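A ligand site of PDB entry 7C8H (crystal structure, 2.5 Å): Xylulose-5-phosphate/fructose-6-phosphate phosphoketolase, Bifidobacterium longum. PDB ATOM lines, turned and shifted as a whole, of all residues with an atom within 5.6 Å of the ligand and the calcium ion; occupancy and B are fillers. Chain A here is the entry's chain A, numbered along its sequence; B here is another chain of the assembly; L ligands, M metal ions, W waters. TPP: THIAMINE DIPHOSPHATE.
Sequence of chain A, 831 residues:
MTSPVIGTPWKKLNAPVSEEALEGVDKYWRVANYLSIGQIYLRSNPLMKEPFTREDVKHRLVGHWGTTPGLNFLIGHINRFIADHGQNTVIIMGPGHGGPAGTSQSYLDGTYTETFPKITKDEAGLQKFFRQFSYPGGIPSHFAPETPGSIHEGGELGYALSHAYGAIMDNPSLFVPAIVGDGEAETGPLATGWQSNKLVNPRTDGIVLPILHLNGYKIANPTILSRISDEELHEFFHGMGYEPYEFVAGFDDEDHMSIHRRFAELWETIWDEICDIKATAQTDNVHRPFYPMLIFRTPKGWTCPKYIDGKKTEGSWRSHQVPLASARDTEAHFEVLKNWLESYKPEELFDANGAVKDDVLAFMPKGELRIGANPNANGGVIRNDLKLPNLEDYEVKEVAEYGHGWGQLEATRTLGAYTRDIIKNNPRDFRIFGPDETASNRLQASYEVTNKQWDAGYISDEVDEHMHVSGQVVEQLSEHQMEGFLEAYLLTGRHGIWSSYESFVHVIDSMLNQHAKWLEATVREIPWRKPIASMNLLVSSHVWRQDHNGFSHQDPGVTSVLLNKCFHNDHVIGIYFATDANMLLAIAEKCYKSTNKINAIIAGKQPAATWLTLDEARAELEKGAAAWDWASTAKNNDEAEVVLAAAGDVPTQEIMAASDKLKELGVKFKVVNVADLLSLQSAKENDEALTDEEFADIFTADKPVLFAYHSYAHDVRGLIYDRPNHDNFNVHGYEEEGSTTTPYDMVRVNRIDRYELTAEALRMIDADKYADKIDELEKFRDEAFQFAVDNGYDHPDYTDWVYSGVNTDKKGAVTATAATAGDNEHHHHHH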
ATOM      1  N   GLY A  66      -0.062  15.451  -4.721  1.00  0.00           N
ATOM      2  CA  GLY A  66      -1.269  15.328  -5.582  1.00  0.00           C
ATOM      3  C   GLY A  66      -1.140  15.976  -6.965  1.00  0.00           C
ATOM      4  O   GLY A  66      -1.320  15.285  -7.987  1.00  0.00           O
ATOM      5  N   THR A  67      -0.869  17.279  -6.983  1.00  0.00           N
ATOM      6  CA  THR A  67      -0.792  18.089  -8.206  1.00  0.00           C
ATOM      7  C   THR A  67       0.455  17.690  -8.999  1.00  0.00           C
ATOM      8  O   THR A  67       0.359  17.630 -10.236  1.00  0.00           O
ATOM      9  CB  THR A  67      -0.871  19.580  -7.849  1.00  0.00           C
ATOM     10  OG1 THR A  67      -1.102  20.246  -9.084  1.00  0.00           O
ATOM     11  CG2 THR A  67       0.374  20.119  -7.195  1.00  0.00           C
ATOM     12  N   PRO A  95      -1.055  25.747  -9.560  1.00  0.00           N
ATOM     13  CA  PRO A  95      -0.865  24.913  -8.390  1.00  0.00           C
ATOM     14  C   PRO A  95       0.565  25.075  -7.848  1.00  0.00           C
ATOM     15  O   PRO A  95       1.382  24.169  -7.925  1.00  0.00           O
ATOM     16  CB  PRO A  95      -1.169  23.484  -8.867  1.00  0.00           C
ATOM     17  CG  PRO A  95      -1.759  23.643 -10.253  1.00  0.00           C
ATOM     18  CD  PRO A  95      -1.242  24.954 -10.784  1.00  0.00           C
ATOM     19  N   HIS A  97       1.821  25.053  -5.041  1.00  0.00           N
ATOM     20  CA  HIS A  97       2.154  24.042  -4.006  1.00  0.00           C
ATOM     21  C   HIS A  97       2.831  22.829  -4.673  1.00  0.00           C
ATOM     22  O   HIS A  97       3.495  22.056  -3.946  1.00  0.00           O
ATOM     23  CB  HIS A  97       0.908  23.748  -3.139  1.00  0.00           C
ATOM     24  CG  HIS A  97      -0.291  23.307  -3.925  1.00  0.00           C
ATOM     25  ND1 HIS A  97      -1.159  24.206  -4.551  1.00  0.00           N
ATOM     26  CD2 HIS A  97      -0.782  22.062  -4.167  1.00  0.00           C
ATOM     27  CE1 HIS A  97      -2.099  23.526  -5.169  1.00  0.00           C
ATOM     28  NE2 HIS A  97      -1.896  22.219  -4.932  1.00  0.00           N
ATOM     29  N   GLY A 154       2.233  30.901  -6.708  1.00  0.00           N
ATOM     30  CA  GLY A 154       1.020  30.071  -6.624  1.00  0.00           C
ATOM     31  C   GLY A 154       0.664  29.684  -5.202  1.00  0.00           C
ATOM     32  O   GLY A 154       0.009  28.585  -5.012  1.00  0.00           O
ATOM     33  N   GLY A 155       1.042  30.536  -4.229  1.00  0.00           N
ATOM     34  CA  GLY A 155       0.789  30.317  -2.794  1.00  0.00           C
ATOM     35  C   GLY A 155      -0.624  30.720  -2.489  1.00  0.00           C
ATOM     36  O   GLY A 155      -1.424  29.895  -2.015  1.00  0.00           O
ATOM     37  N   GLU A 156      -0.957  31.971  -2.776  1.00  0.00           N
ATOM     38  CA  GLU A 156      -2.346  32.430  -2.721  1.00  0.00           C
ATOM     39  C   GLU A 156      -2.912  32.167  -4.106  1.00  0.00           C
ATOM     40  O   GLU A 156      -2.462  32.849  -5.051  1.00  0.00           O
ATOM     41  CB  GLU A 156      -2.415  33.886  -2.301  1.00  0.00           C
ATOM     42  CG  GLU A 156      -3.822  34.334  -1.938  1.00  0.00           C
ATOM     43  CD  GLU A 156      -3.796  35.757  -1.413  1.00  0.00           C
ATOM     44  OE1 GLU A 156      -3.117  35.973  -0.388  1.00  0.00           O
ATOM     45  OE2 GLU A 156      -4.354  36.646  -2.097  1.00  0.00           O
ATOM     46  N   LEU A 157      -3.823  31.197  -4.198  1.00  0.00           N
ATOM     47  CA  LEU A 157      -4.449  30.736  -5.458  1.00  0.00           C
ATOM     48  C   LEU A 157      -5.327  31.841  -6.033  1.00  0.00           C
ATOM     49  O   LEU A 157      -5.965  32.541  -5.248  1.00  0.00           O
ATOM     50  CB  LEU A 157      -5.277  29.494  -5.176  1.00  0.00           C
ATOM     51  CG  LEU A 157      -4.448  28.257  -4.837  1.00  0.00           C
ATOM     52  CD1 LEU A 157      -5.361  27.064  -4.605  1.00  0.00           C
ATOM     53  CD2 LEU A 157      -3.429  27.960  -5.930  1.00  0.00           C
ATOM     54  N   TYR A 159      -4.411  33.758  -9.263  1.00  0.00           N
ATOM     55  CA  TYR A 159      -3.781  34.816 -10.104  1.00  0.00           C
ATOM     56  C   TYR A 159      -3.077  34.181 -11.297  1.00  0.00           C
ATOM     57  O   TYR A 159      -2.279  34.854 -11.978  1.00  0.00           O
ATOM     58  CB  TYR A 159      -2.875  35.669  -9.219  1.00  0.00           C
ATOM     59  CG  TYR A 159      -3.537  35.972  -7.902  1.00  0.00           C
ATOM     60  CD1 TYR A 159      -4.803  36.522  -7.839  1.00  0.00           C
ATOM     61  CD2 TYR A 159      -2.922  35.654  -6.718  1.00  0.00           C
ATOM     62  CE1 TYR A 159      -5.442  36.738  -6.636  1.00  0.00           C
ATOM     63  CE2 TYR A 159      -3.550  35.860  -5.499  1.00  0.00           C
ATOM     64  CZ  TYR A 159      -4.819  36.399  -5.446  1.00  0.00           C
ATOM     65  OH  TYR A 159      -5.414  36.578  -4.237  1.00  0.00           O
ATOM     66  N   GLY A 181      -5.190  25.176 -11.396  1.00  0.00           N
ATOM     67  CA  GLY A 181      -5.817  24.157 -10.543  1.00  0.00           C
ATOM     68  C   GLY A 181      -7.336  24.163 -10.700  1.00  0.00           C
ATOM     69  O   GLY A 181      -7.902  25.240 -10.941  1.00  0.00           O
ATOM     70  N   ASP A 182      -7.982  23.004 -10.602  1.00  0.00           N
ATOM     71  CA  ASP A 182      -9.446  22.913 -10.750  1.00  0.00           C
ATOM     72  C   ASP A 182     -10.105  23.484  -9.482  1.00  0.00           C
ATOM     73  O   ASP A 182     -11.187  24.036  -9.619  1.00  0.00           O
ATOM     74  CB  ASP A 182      -9.900  21.511 -11.214  1.00  0.00           C
ATOM     75  CG  ASP A 182      -9.515  20.338 -10.338  1.00  0.00           C
ATOM     76  OD1 ASP A 182      -8.620  20.503  -9.548  1.00  0.00           O
ATOM     77  OD2 ASP A 182     -10.131  19.245 -10.481  1.00  0.00           O
ATOM     78  N   GLY A 183      -9.455  23.412  -8.321  1.00  0.00           N
ATOM     79  CA  GLY A 183      -9.812  24.151  -7.084  1.00  0.00           C
ATOM     80  C   GLY A 183      -9.532  25.655  -7.193  1.00  0.00           C
ATOM     81  O   GLY A 183     -10.434  26.460  -6.876  1.00  0.00           O
ATOM     82  N   GLU A 184      -8.338  26.044  -7.631  1.00  0.00           N
ATOM     83  CA  GLU A 184      -8.020  27.450  -7.947  1.00  0.00           C
ATOM     84  C   GLU A 184      -9.144  28.022  -8.841  1.00  0.00           C
ATOM     85  O   GLU A 184      -9.527  29.180  -8.625  1.00  0.00           O
ATOM     86  CB  GLU A 184      -6.637  27.552  -8.601  1.00  0.00           C
ATOM     87  CG  GLU A 184      -6.251  28.961  -8.997  1.00  0.00           C
ATOM     88  CD  GLU A 184      -4.854  29.096  -9.564  1.00  0.00           C
ATOM     89  OE1 GLU A 184      -4.324  28.103 -10.115  1.00  0.00           O
ATOM     90  OE2 GLU A 184      -4.300  30.188  -9.464  1.00  0.00           O
ATOM     91  N   ALA A 185      -9.686  27.234  -9.778  1.00  0.00           N
ATOM     92  CA  ALA A 185     -10.741  27.685 -10.722  1.00  0.00           C
ATOM     93  C   ALA A 185     -12.004  28.168  -9.974  1.00  0.00           C
ATOM     94  O   ALA A 185     -12.803  28.910 -10.581  1.00  0.00           O
ATOM     95  CB  ALA A 185     -11.079  26.603 -11.684  1.00  0.00           C
ATOM     96  N   THR A 187     -11.900  30.096  -7.219  1.00  0.00           N
ATOM     97  CA  THR A 187     -11.653  31.439  -6.625  1.00  0.00           C
ATOM     98  C   THR A 187     -12.292  32.429  -7.585  1.00  0.00           C
ATOM     99  O   THR A 187     -12.462  32.056  -8.764  1.00  0.00           O
ATOM    100  CB  THR A 187     -10.179  31.791  -6.459  1.00  0.00           C
ATOM    101  OG1 THR A 187      -9.547  31.774  -7.744  1.00  0.00           O
ATOM    102  CG2 THR A 187      -9.428  30.846  -5.558  1.00  0.00           C
ATOM    103  N   HIS A 213      -5.813  21.835 -14.871  1.00  0.00           N
ATOM    104  CA  HIS A 213      -5.345  20.642 -14.133  1.00  0.00           C
ATOM    105  C   HIS A 213      -6.566  20.016 -13.452  1.00  0.00           C
ATOM    106  O   HIS A 213      -6.745  20.132 -12.203  1.00  0.00           O
ATOM    107  CB  HIS A 213      -4.182  21.082 -13.253  1.00  0.00           C
ATOM    108  CG  HIS A 213      -3.398  19.959 -12.678  1.00  0.00           C
ATOM    109  ND1 HIS A 213      -3.539  18.670 -13.111  1.00  0.00           N
ATOM    110  CD2 HIS A 213      -2.445  19.952 -11.720  1.00  0.00           C
ATOM    111  CE1 HIS A 213      -2.726  17.902 -12.431  1.00  0.00           C
ATOM    112  NE2 HIS A 213      -2.017  18.683 -11.589  1.00  0.00           N
ATOM    113  N   ASN A 215      -7.825  17.515 -11.966  1.00  0.00           N
ATOM    114  CA  ASN A 215      -7.469  16.266 -11.266  1.00  0.00           C
ATOM    115  C   ASN A 215      -8.574  15.910 -10.266  1.00  0.00           C
ATOM    116  O   ASN A 215      -8.374  15.031  -9.449  1.00  0.00           O
ATOM    117  CB  ASN A 215      -6.060  16.360 -10.678  1.00  0.00           C
ATOM    118  CG  ASN A 215      -5.966  17.435  -9.631  1.00  0.00           C
ATOM    119  OD1 ASN A 215      -6.986  17.892  -9.147  1.00  0.00           O
ATOM    120  ND2 ASN A 215      -4.756  17.852  -9.304  1.00  0.00           N
ATOM    121  N   GLY A 216      -9.731  16.581 -10.327  1.00  0.00           N
ATOM    122  CA  GLY A 216     -10.965  16.099  -9.690  1.00  0.00           C
ATOM    123  C   GLY A 216     -11.133  16.561  -8.254  1.00  0.00           C
ATOM    124  O   GLY A 216     -12.253  16.402  -7.723  1.00  0.00           O
ATOM    125  N   TYR A 217     -10.088  17.096  -7.615  1.00  0.00           N
ATOM    126  CA  TYR A 217     -10.046  17.300  -6.147  1.00  0.00           C
ATOM    127  C   TYR A 217      -9.202  18.506  -5.847  1.00  0.00           C
ATOM    128  O   TYR A 217      -8.393  18.923  -6.678  1.00  0.00           O
ATOM    129  CB  TYR A 217      -9.549  16.057  -5.394  1.00  0.00           C
ATOM    130  CG  TYR A 217     -10.431  14.860  -5.622  1.00  0.00           C
ATOM    131  CD1 TYR A 217     -11.629  14.730  -4.944  1.00  0.00           C
ATOM    132  CD2 TYR A 217     -10.151  13.963  -6.639  1.00  0.00           C
ATOM    133  CE1 TYR A 217     -12.485  13.683  -5.229  1.00  0.00           C
ATOM    134  CE2 TYR A 217     -11.003  12.907  -6.938  1.00  0.00           C
ATOM    135  CZ  TYR A 217     -12.179  12.775  -6.227  1.00  0.00           C
ATOM    136  OH  TYR A 217     -13.009  11.739  -6.505  1.00  0.00           O
ATOM    137  N   LYS A 218      -9.527  19.107  -4.720  1.00  0.00           N
ATOM    138  CA  LYS A 218      -8.794  20.189  -4.058  1.00  0.00           C
ATOM    139  C   LYS A 218      -8.313  19.528  -2.768  1.00  0.00           C
ATOM    140  O   LYS A 218      -7.917  18.350  -2.874  1.00  0.00           O
ATOM    141  CB  LYS A 218      -9.651  21.463  -3.962  1.00  0.00           C
ATOM    142  CG  LYS A 218     -11.132  21.321  -3.602  1.00  0.00           C
ATOM    143  CD  LYS A 218     -11.844  22.654  -3.584  1.00  0.00           C
ATOM    144  CE  LYS A 218     -13.269  22.613  -3.078  1.00  0.00           C
ATOM    145  NZ  LYS A 218     -14.236  22.247  -4.139  1.00  0.00           N
ATOM    146  N   ILE A 219      -8.343  20.190  -1.614  1.00  0.00           N
ATOM    147  CA  ILE A 219      -7.752  19.593  -0.380  1.00  0.00           C
ATOM    148  C   ILE A 219      -8.567  18.369   0.037  1.00  0.00           C
ATOM    149  O   ILE A 219      -7.970  17.285   0.175  1.00  0.00           O
ATOM    150  CB  ILE A 219      -7.676  20.596   0.770  1.00  0.00           C
ATOM    151  CG1 ILE A 219      -6.745  21.771   0.431  1.00  0.00           C
ATOM    152  CG2 ILE A 219      -7.233  19.855   2.021  1.00  0.00           C
ATOM    153  CD1 ILE A 219      -6.911  22.948   1.352  1.00  0.00           C
ATOM    154  N   THR A 223     -13.870  18.948  -6.927  1.00  0.00           N
ATOM    155  CA  THR A 223     -13.945  20.296  -7.481  1.00  0.00           C
ATOM    156  C   THR A 223     -15.232  20.381  -8.270  1.00  0.00           C
ATOM    157  O   THR A 223     -15.591  19.400  -8.941  1.00  0.00           O
ATOM    158  CB  THR A 223     -12.710  20.576  -8.330  1.00  0.00           C
ATOM    159  OG1 THR A 223     -12.564  19.464  -9.211  1.00  0.00           O
ATOM    160  CG2 THR A 223     -11.489  20.800  -7.462  1.00  0.00           C
ATOM    161  N   LYS A 300      -5.783  12.639  -9.483  1.00  0.00           N
ATOM    162  CA  LYS A 300      -4.967  13.417  -8.531  1.00  0.00           C
ATOM    163  C   LYS A 300      -4.027  12.427  -7.849  1.00  0.00           C
ATOM    164  O   LYS A 300      -4.511  11.363  -7.457  1.00  0.00           O
ATOM    165  CB  LYS A 300      -5.804  14.157  -7.487  1.00  0.00           C
ATOM    166  CG  LYS A 300      -4.984  15.082  -6.590  1.00  0.00           C
ATOM    167  CD  LYS A 300      -5.718  16.300  -6.029  1.00  0.00           C
ATOM    168  CE  LYS A 300      -4.867  17.136  -5.121  1.00  0.00           C
ATOM    169  NZ  LYS A 300      -5.547  18.344  -4.629  1.00  0.00           N
ATOM    170  N   HIS A 320      -3.476  14.799  -1.711  1.00  0.00           N
ATOM    171  CA  HIS A 320      -3.261  16.234  -1.996  1.00  0.00           C
ATOM    172  C   HIS A 320      -1.943  16.689  -1.357  1.00  0.00           C
ATOM    173  O   HIS A 320      -1.144  17.384  -2.049  1.00  0.00           O
ATOM    174  CB  HIS A 320      -4.450  17.074  -1.541  1.00  0.00           C
ATOM    175  CG  HIS A 320      -4.112  18.512  -1.441  1.00  0.00           C
ATOM    176  ND1 HIS A 320      -4.014  19.303  -2.560  1.00  0.00           N
ATOM    177  CD2 HIS A 320      -3.808  19.289  -0.375  1.00  0.00           C
ATOM    178  CE1 HIS A 320      -3.652  20.525  -2.188  1.00  0.00           C
ATOM    179  NE2 HIS A 320      -3.556  20.544  -0.847  1.00  0.00           N
ATOM    180  N   PRO B 435     -13.512  27.617   2.917  1.00  0.00           N
ATOM    181  CA  PRO B 435     -12.925  27.540   1.588  1.00  0.00           C
ATOM    182  C   PRO B 435     -12.103  26.271   1.419  1.00  0.00           C
ATOM    183  O   PRO B 435     -10.917  26.387   1.283  1.00  0.00           O
ATOM    184  CB  PRO B 435     -12.024  28.775   1.532  1.00  0.00           C
ATOM    185  CG  PRO B 435     -12.270  29.497   2.828  1.00  0.00           C
ATOM    186  CD  PRO B 435     -12.706  28.440   3.807  1.00  0.00           C
ATOM    187  N   ASP B 436     -12.764  25.103   1.490  1.00  0.00           N
ATOM    188  CA  ASP B 436     -12.135  23.751   1.393  1.00  0.00           C
ATOM    189  C   ASP B 436     -11.227  23.534   2.609  1.00  0.00           C
ATOM    190  O   ASP B 436     -10.234  22.819   2.475  1.00  0.00           O
ATOM    191  CB  ASP B 436     -11.427  23.606   0.031  1.00  0.00           C
ATOM    192  CG  ASP B 436     -10.842  22.242  -0.288  1.00  0.00           C
ATOM    193  OD1 ASP B 436     -11.425  21.176   0.155  1.00  0.00           O
ATOM    194  OD2 ASP B 436      -9.807  22.250  -0.985  1.00  0.00           O
ATOM    195  N   GLU B 437     -11.548  24.154   3.746  1.00  0.00           N
ATOM    196  CA  GLU B 437     -10.655  24.221   4.924  1.00  0.00           C
ATOM    197  C   GLU B 437     -11.371  23.809   6.206  1.00  0.00           C
ATOM    198  O   GLU B 437     -10.718  23.907   7.278  1.00  0.00           O
ATOM    199  CB  GLU B 437     -10.100  25.642   5.062  1.00  0.00           C
ATOM    200  CG  GLU B 437      -9.095  26.018   3.985  1.00  0.00           C
ATOM    201  CD  GLU B 437      -8.741  27.495   4.005  1.00  0.00           C
ATOM    202  OE1 GLU B 437      -8.925  28.114   5.055  1.00  0.00           O
ATOM    203  OE2 GLU B 437      -8.328  28.031   2.970  1.00  0.00           O
ATOM    204  N   LEU B 477     -13.748  26.688  -2.987  1.00  0.00           N
ATOM    205  CA  LEU B 477     -12.432  27.356  -2.776  1.00  0.00           C
ATOM    206  C   LEU B 477     -12.586  28.817  -3.203  1.00  0.00           C
ATOM    207  O   LEU B 477     -12.140  29.201  -4.315  1.00  0.00           O
ATOM    208  CB  LEU B 477     -11.328  26.575  -3.483  1.00  0.00           C
ATOM    209  CG  LEU B 477      -9.882  27.090  -3.457  1.00  0.00           C
ATOM    210  CD1 LEU B 477      -9.561  28.043  -2.324  1.00  0.00           C
ATOM    211  CD2 LEU B 477      -8.929  25.905  -3.457  1.00  0.00           C
ATOM    212  N   GLU B 479     -12.917  32.410  -0.615  1.00  0.00           N
ATOM    213  CA  GLU B 479     -13.152  33.275   0.561  1.00  0.00           C
ATOM    214  C   GLU B 479     -14.327  34.220   0.252  1.00  0.00           C
ATOM    215  O   GLU B 479     -15.143  34.452   1.141  1.00  0.00           O
ATOM    216  CB  GLU B 479     -11.861  34.009   0.898  1.00  0.00           C
ATOM    217  CG  GLU B 479     -10.759  33.094   1.363  1.00  0.00           C
ATOM    218  CD  GLU B 479      -9.955  32.343   0.302  1.00  0.00           C
ATOM    219  OE1 GLU B 479     -10.041  32.707  -0.921  1.00  0.00           O
ATOM    220  OE2 GLU B 479      -9.243  31.383   0.705  1.00  0.00           O
ATOM    221  N   TYR B 501      -7.755  29.907   6.849  1.00  0.00           N
ATOM    222  CA  TYR B 501      -6.313  30.162   7.055  1.00  0.00           C
ATOM    223  C   TYR B 501      -6.185  31.670   7.197  1.00  0.00           C
ATOM    224  O   TYR B 501      -6.761  32.438   6.401  1.00  0.00           O
ATOM    225  CB  TYR B 501      -5.463  29.647   5.893  1.00  0.00           C
ATOM    226  CG  TYR B 501      -5.546  28.166   5.604  1.00  0.00           C
ATOM    227  CD1 TYR B 501      -6.157  27.260   6.452  1.00  0.00           C
ATOM    228  CD2 TYR B 501      -4.953  27.670   4.453  1.00  0.00           C
ATOM    229  CE1 TYR B 501      -6.174  25.906   6.162  1.00  0.00           C
ATOM    230  CE2 TYR B 501      -4.987  26.327   4.139  1.00  0.00           C
ATOM    231  CZ  TYR B 501      -5.589  25.430   5.005  1.00  0.00           C
ATOM    232  OH  TYR B 501      -5.575  24.106   4.638  1.00  0.00           O
ATOM    233  N   PHE B 504      -5.184  34.134   4.223  1.00  0.00           N
ATOM    234  CA  PHE B 504      -6.144  34.288   3.098  1.00  0.00           C
ATOM    235  C   PHE B 504      -7.440  35.022   3.510  1.00  0.00           C
ATOM    236  O   PHE B 504      -8.260  35.339   2.588  1.00  0.00           O
ATOM    237  CB  PHE B 504      -6.396  32.918   2.471  1.00  0.00           C
ATOM    238  CG  PHE B 504      -5.114  32.278   2.002  1.00  0.00           C
ATOM    239  CD1 PHE B 504      -4.122  33.030   1.401  1.00  0.00           C
ATOM    240  CD2 PHE B 504      -4.893  30.926   2.201  1.00  0.00           C
ATOM    241  CE1 PHE B 504      -2.935  32.445   1.019  1.00  0.00           C
ATOM    242  CE2 PHE B 504      -3.704  30.353   1.806  1.00  0.00           C
ATOM    243  CZ  PHE B 504      -2.735  31.112   1.209  1.00  0.00           C
ATOM    244  N   VAL B 507      -7.935  38.058   1.520  1.00  0.00           N
ATOM    245  CA  VAL B 507      -8.711  38.000   0.244  1.00  0.00           C
ATOM    246  C   VAL B 507     -10.039  38.756   0.404  1.00  0.00           C
ATOM    247  O   VAL B 507     -10.469  39.438  -0.537  1.00  0.00           O
ATOM    248  CB  VAL B 507      -8.923  36.557  -0.222  1.00  0.00           C
ATOM    249  CG1 VAL B 507      -9.994  36.467  -1.311  1.00  0.00           C
ATOM    250  CG2 VAL B 507      -7.622  35.973  -0.725  1.00  0.00           C
ATOM    251  N   HIS B 553       1.936  32.183   3.212  1.00  0.00           N
ATOM    252  CA  HIS B 553       0.823  31.844   4.147  1.00  0.00           C
ATOM    253  C   HIS B 553       1.011  32.597   5.475  1.00  0.00           C
ATOM    254  O   HIS B 553       0.237  32.335   6.398  1.00  0.00           O
ATOM    255  CB  HIS B 553       0.751  30.318   4.335  1.00  0.00           C
ATOM    256  CG  HIS B 553       0.210  29.594   3.151  1.00  0.00           C
ATOM    257  ND1 HIS B 553       0.712  29.777   1.876  1.00  0.00           N
ATOM    258  CD2 HIS B 553      -0.768  28.659   3.056  1.00  0.00           C
ATOM    259  CE1 HIS B 553       0.054  29.012   1.026  1.00  0.00           C
ATOM    260  NE2 HIS B 553      -0.869  28.307   1.727  1.00  0.00           N
HETATM  261  N1' TPP L   1      -7.485  30.106  -0.396  1.00  0.00           N
HETATM  262  C2' TPP L   1      -6.561  30.715  -1.137  1.00  0.00           C
HETATM  263  CM2 TPP L   1      -6.911  32.027  -1.756  1.00  0.00           C
HETATM  264  N3' TPP L   1      -5.349  30.231  -1.401  1.00  0.00           N
HETATM  265  C4' TPP L   1      -5.026  29.063  -0.830  1.00  0.00           C
HETATM  266  N4' TPP L   1      -3.791  28.627  -1.046  1.00  0.00           N
HETATM  267  C5' TPP L   1      -5.945  28.340  -0.050  1.00  0.00           C
HETATM  268  C6' TPP L   1      -7.173  28.921   0.134  1.00  0.00           C
HETATM  269  C7' TPP L   1      -5.618  27.008   0.547  1.00  0.00           C
HETATM  270  N3  TPP L   1      -5.371  25.999  -0.490  1.00  0.00           N
HETATM  271  C2  TPP L   1      -4.131  25.726  -0.927  1.00  0.00           C
HETATM  272  S1  TPP L   1      -4.117  24.360  -1.998  1.00  0.00           S
HETATM  273  C5  TPP L   1      -5.839  24.296  -1.909  1.00  0.00           C
HETATM  274  C4  TPP L   1      -6.346  25.176  -1.009  1.00  0.00           C
HETATM  275  CM4 TPP L   1      -7.759  25.302  -0.539  1.00  0.00           C
HETATM  276  C6  TPP L   1      -6.560  23.360  -2.821  1.00  0.00           C
HETATM  277  C7  TPP L   1      -6.146  23.611  -4.239  1.00  0.00           C
HETATM  278  O7  TPP L   1      -6.653  22.587  -5.115  1.00  0.00           O
HETATM  279  PA  TPP L   1      -6.375  22.740  -6.675  1.00  0.00           P
HETATM  280  O1A TPP L   1      -7.414  21.892  -7.298  1.00  0.00           O
HETATM  281  O2A TPP L   1      -6.207  24.110  -7.254  1.00  0.00           O
HETATM  282  O3A TPP L   1      -4.930  22.026  -6.659  1.00  0.00           O
HETATM  283  PB  TPP L   1      -4.337  20.533  -6.882  1.00  0.00           P
HETATM  284  O1B TPP L   1      -3.643  20.695  -8.198  1.00  0.00           O
HETATM  285  O2B TPP L   1      -5.400  19.468  -6.952  1.00  0.00           O
HETATM  286  O3B TPP L   1      -3.448  20.277  -5.704  1.00  0.00           O
HETATM  287 CA    CA M   1      -6.966  19.968  -8.184  1.00  0.00          CA
HETATM  288  O   HOH W   1      -5.566  20.824  -9.849  1.00  0.00           O
HETATM  289  O   HOH W   2      -1.660  18.586  -4.479  1.00  0.00           O
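The calcium ion is bound by an oxygen (O2B) of the ligand (2.1 Å), an oxygen (O1A) of the ligand (2.2 Å), the side-chain carboxylate of Asp 182 (2.2 Å), the side-chain amide oxygen of Asn 215 (2.3 Å), the backbone carbonyl oxygen of Tyr 217 (2.3 Å) and water W1 (2.3 Å).
Water W1 lies within hydrogen-bond range of O1B of the ligand, O of His 213, ND2 of Asn 215 and N of Asp 182. Water W2 lies within hydrogen-bond range of an oxygen (O3B) of the ligand (2.7 Å), the backbone carbonyl oxygen of His 320 (2.8 Å) and the backbone NH of Thr 67 (2.9 Å).
Residues that only touch the ligand: Pro 95, Glu 156, Gly 181, His 213, Lys 218, Ile 219, Pro 435 of chain B, Asp 436 of chain B, Glu 437 of chain B, Leu 477 of chain B, Tyr 501 of chain B and Phe 504 of chain B. Hydrophobic or aromatic side chains within 4 Å of the ligand: Pro 95, His 97, Leu 157, His 213, Ile 219, His 320, Leu 477 of chain B, Tyr 501 of chain B and Phe 504 of chain B. Of the 33 residues printed, 24 come within 4 Å of the ligand.
The side-chain carboxylate (OD2) of Asp 182 sits at hydrogen-bond distance from the side-chain hydroxyl (OG1) of Thr 223, 2.8 Å away. N of Gly 216 lies within hydrogen-bond range of OD2 of Asp 182 (2.7 Å). NZ of Lys 300 sits at hydrogen-bond distance from ND1 of His 320. The side-chain amino group (NZ) of Lys 300 is in hydrogen-bond range of the backbone carbonyl oxygen (O) of Lys 218 (2.9 Å). A ring nitrogen (NE2) of His 213 is in hydrogen-bond range of the backbone carbonyl oxygen (O) of Thr 67, at 2.9 Å. The side-chain carboxylate (OE1) of Glu 184 sits at hydrogen-bond distance from the backbone NH (N) of Gly 181 (3.3 Å). The side-chain carboxylate (OD2) of Asp 436 of chain B lies within hydrogen-bond range of the backbone NH (N) of Ile 219, at 2.6 Å. The backbone carbonyl oxygen (O) of His 320 is in hydrogen-bond range of the backbone NH (N) of Gly 66 (3.5 Å).
Three residues have an atom within 4 Å of the calcium ion: Asp 182, Asn 215 and Tyr 217. The nearest printed residue that does not touch the calcium ion is His 213 (4.03 Å).
OE2 of Glu 479 of chain B lies within hydrogen-bond range of N1' of the ligand. The side-chain amino group (NZ) of Lys 300 is in salt-bridge range of an oxygen (O3B) of the ligand (3.0 Å). A ring nitrogen (NE2) of His 97 sits at hydrogen-bond distance from an oxygen (O3B) of the ligand, 2.6 Å away. OG1 of Thr 67 lies within hydrogen-bond range of O1B of the ligand, at 2.7 Å. An oxygen (O2A) of the ligand sits at hydrogen-bond distance from the backbone NH (N) of Gly 183, 3.5 Å away. The backbone carbonyl oxygen of Gly 155 sits at hydrogen-bond distance from a nitrogen (N4') of the ligand (2.9 Å). N of Glu 184 is in hydrogen-bond range of O2A of the ligand (2.9 Å). The backbone NH (N) of Leu 157 sits at hydrogen-bond distance from a nitrogen (N3') of the ligand (3.3 Å). A ring nitrogen (ND1) of His 320 is in hydrogen-bond range of an oxygen (O3B) of the ligand, at 3.3 Å.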
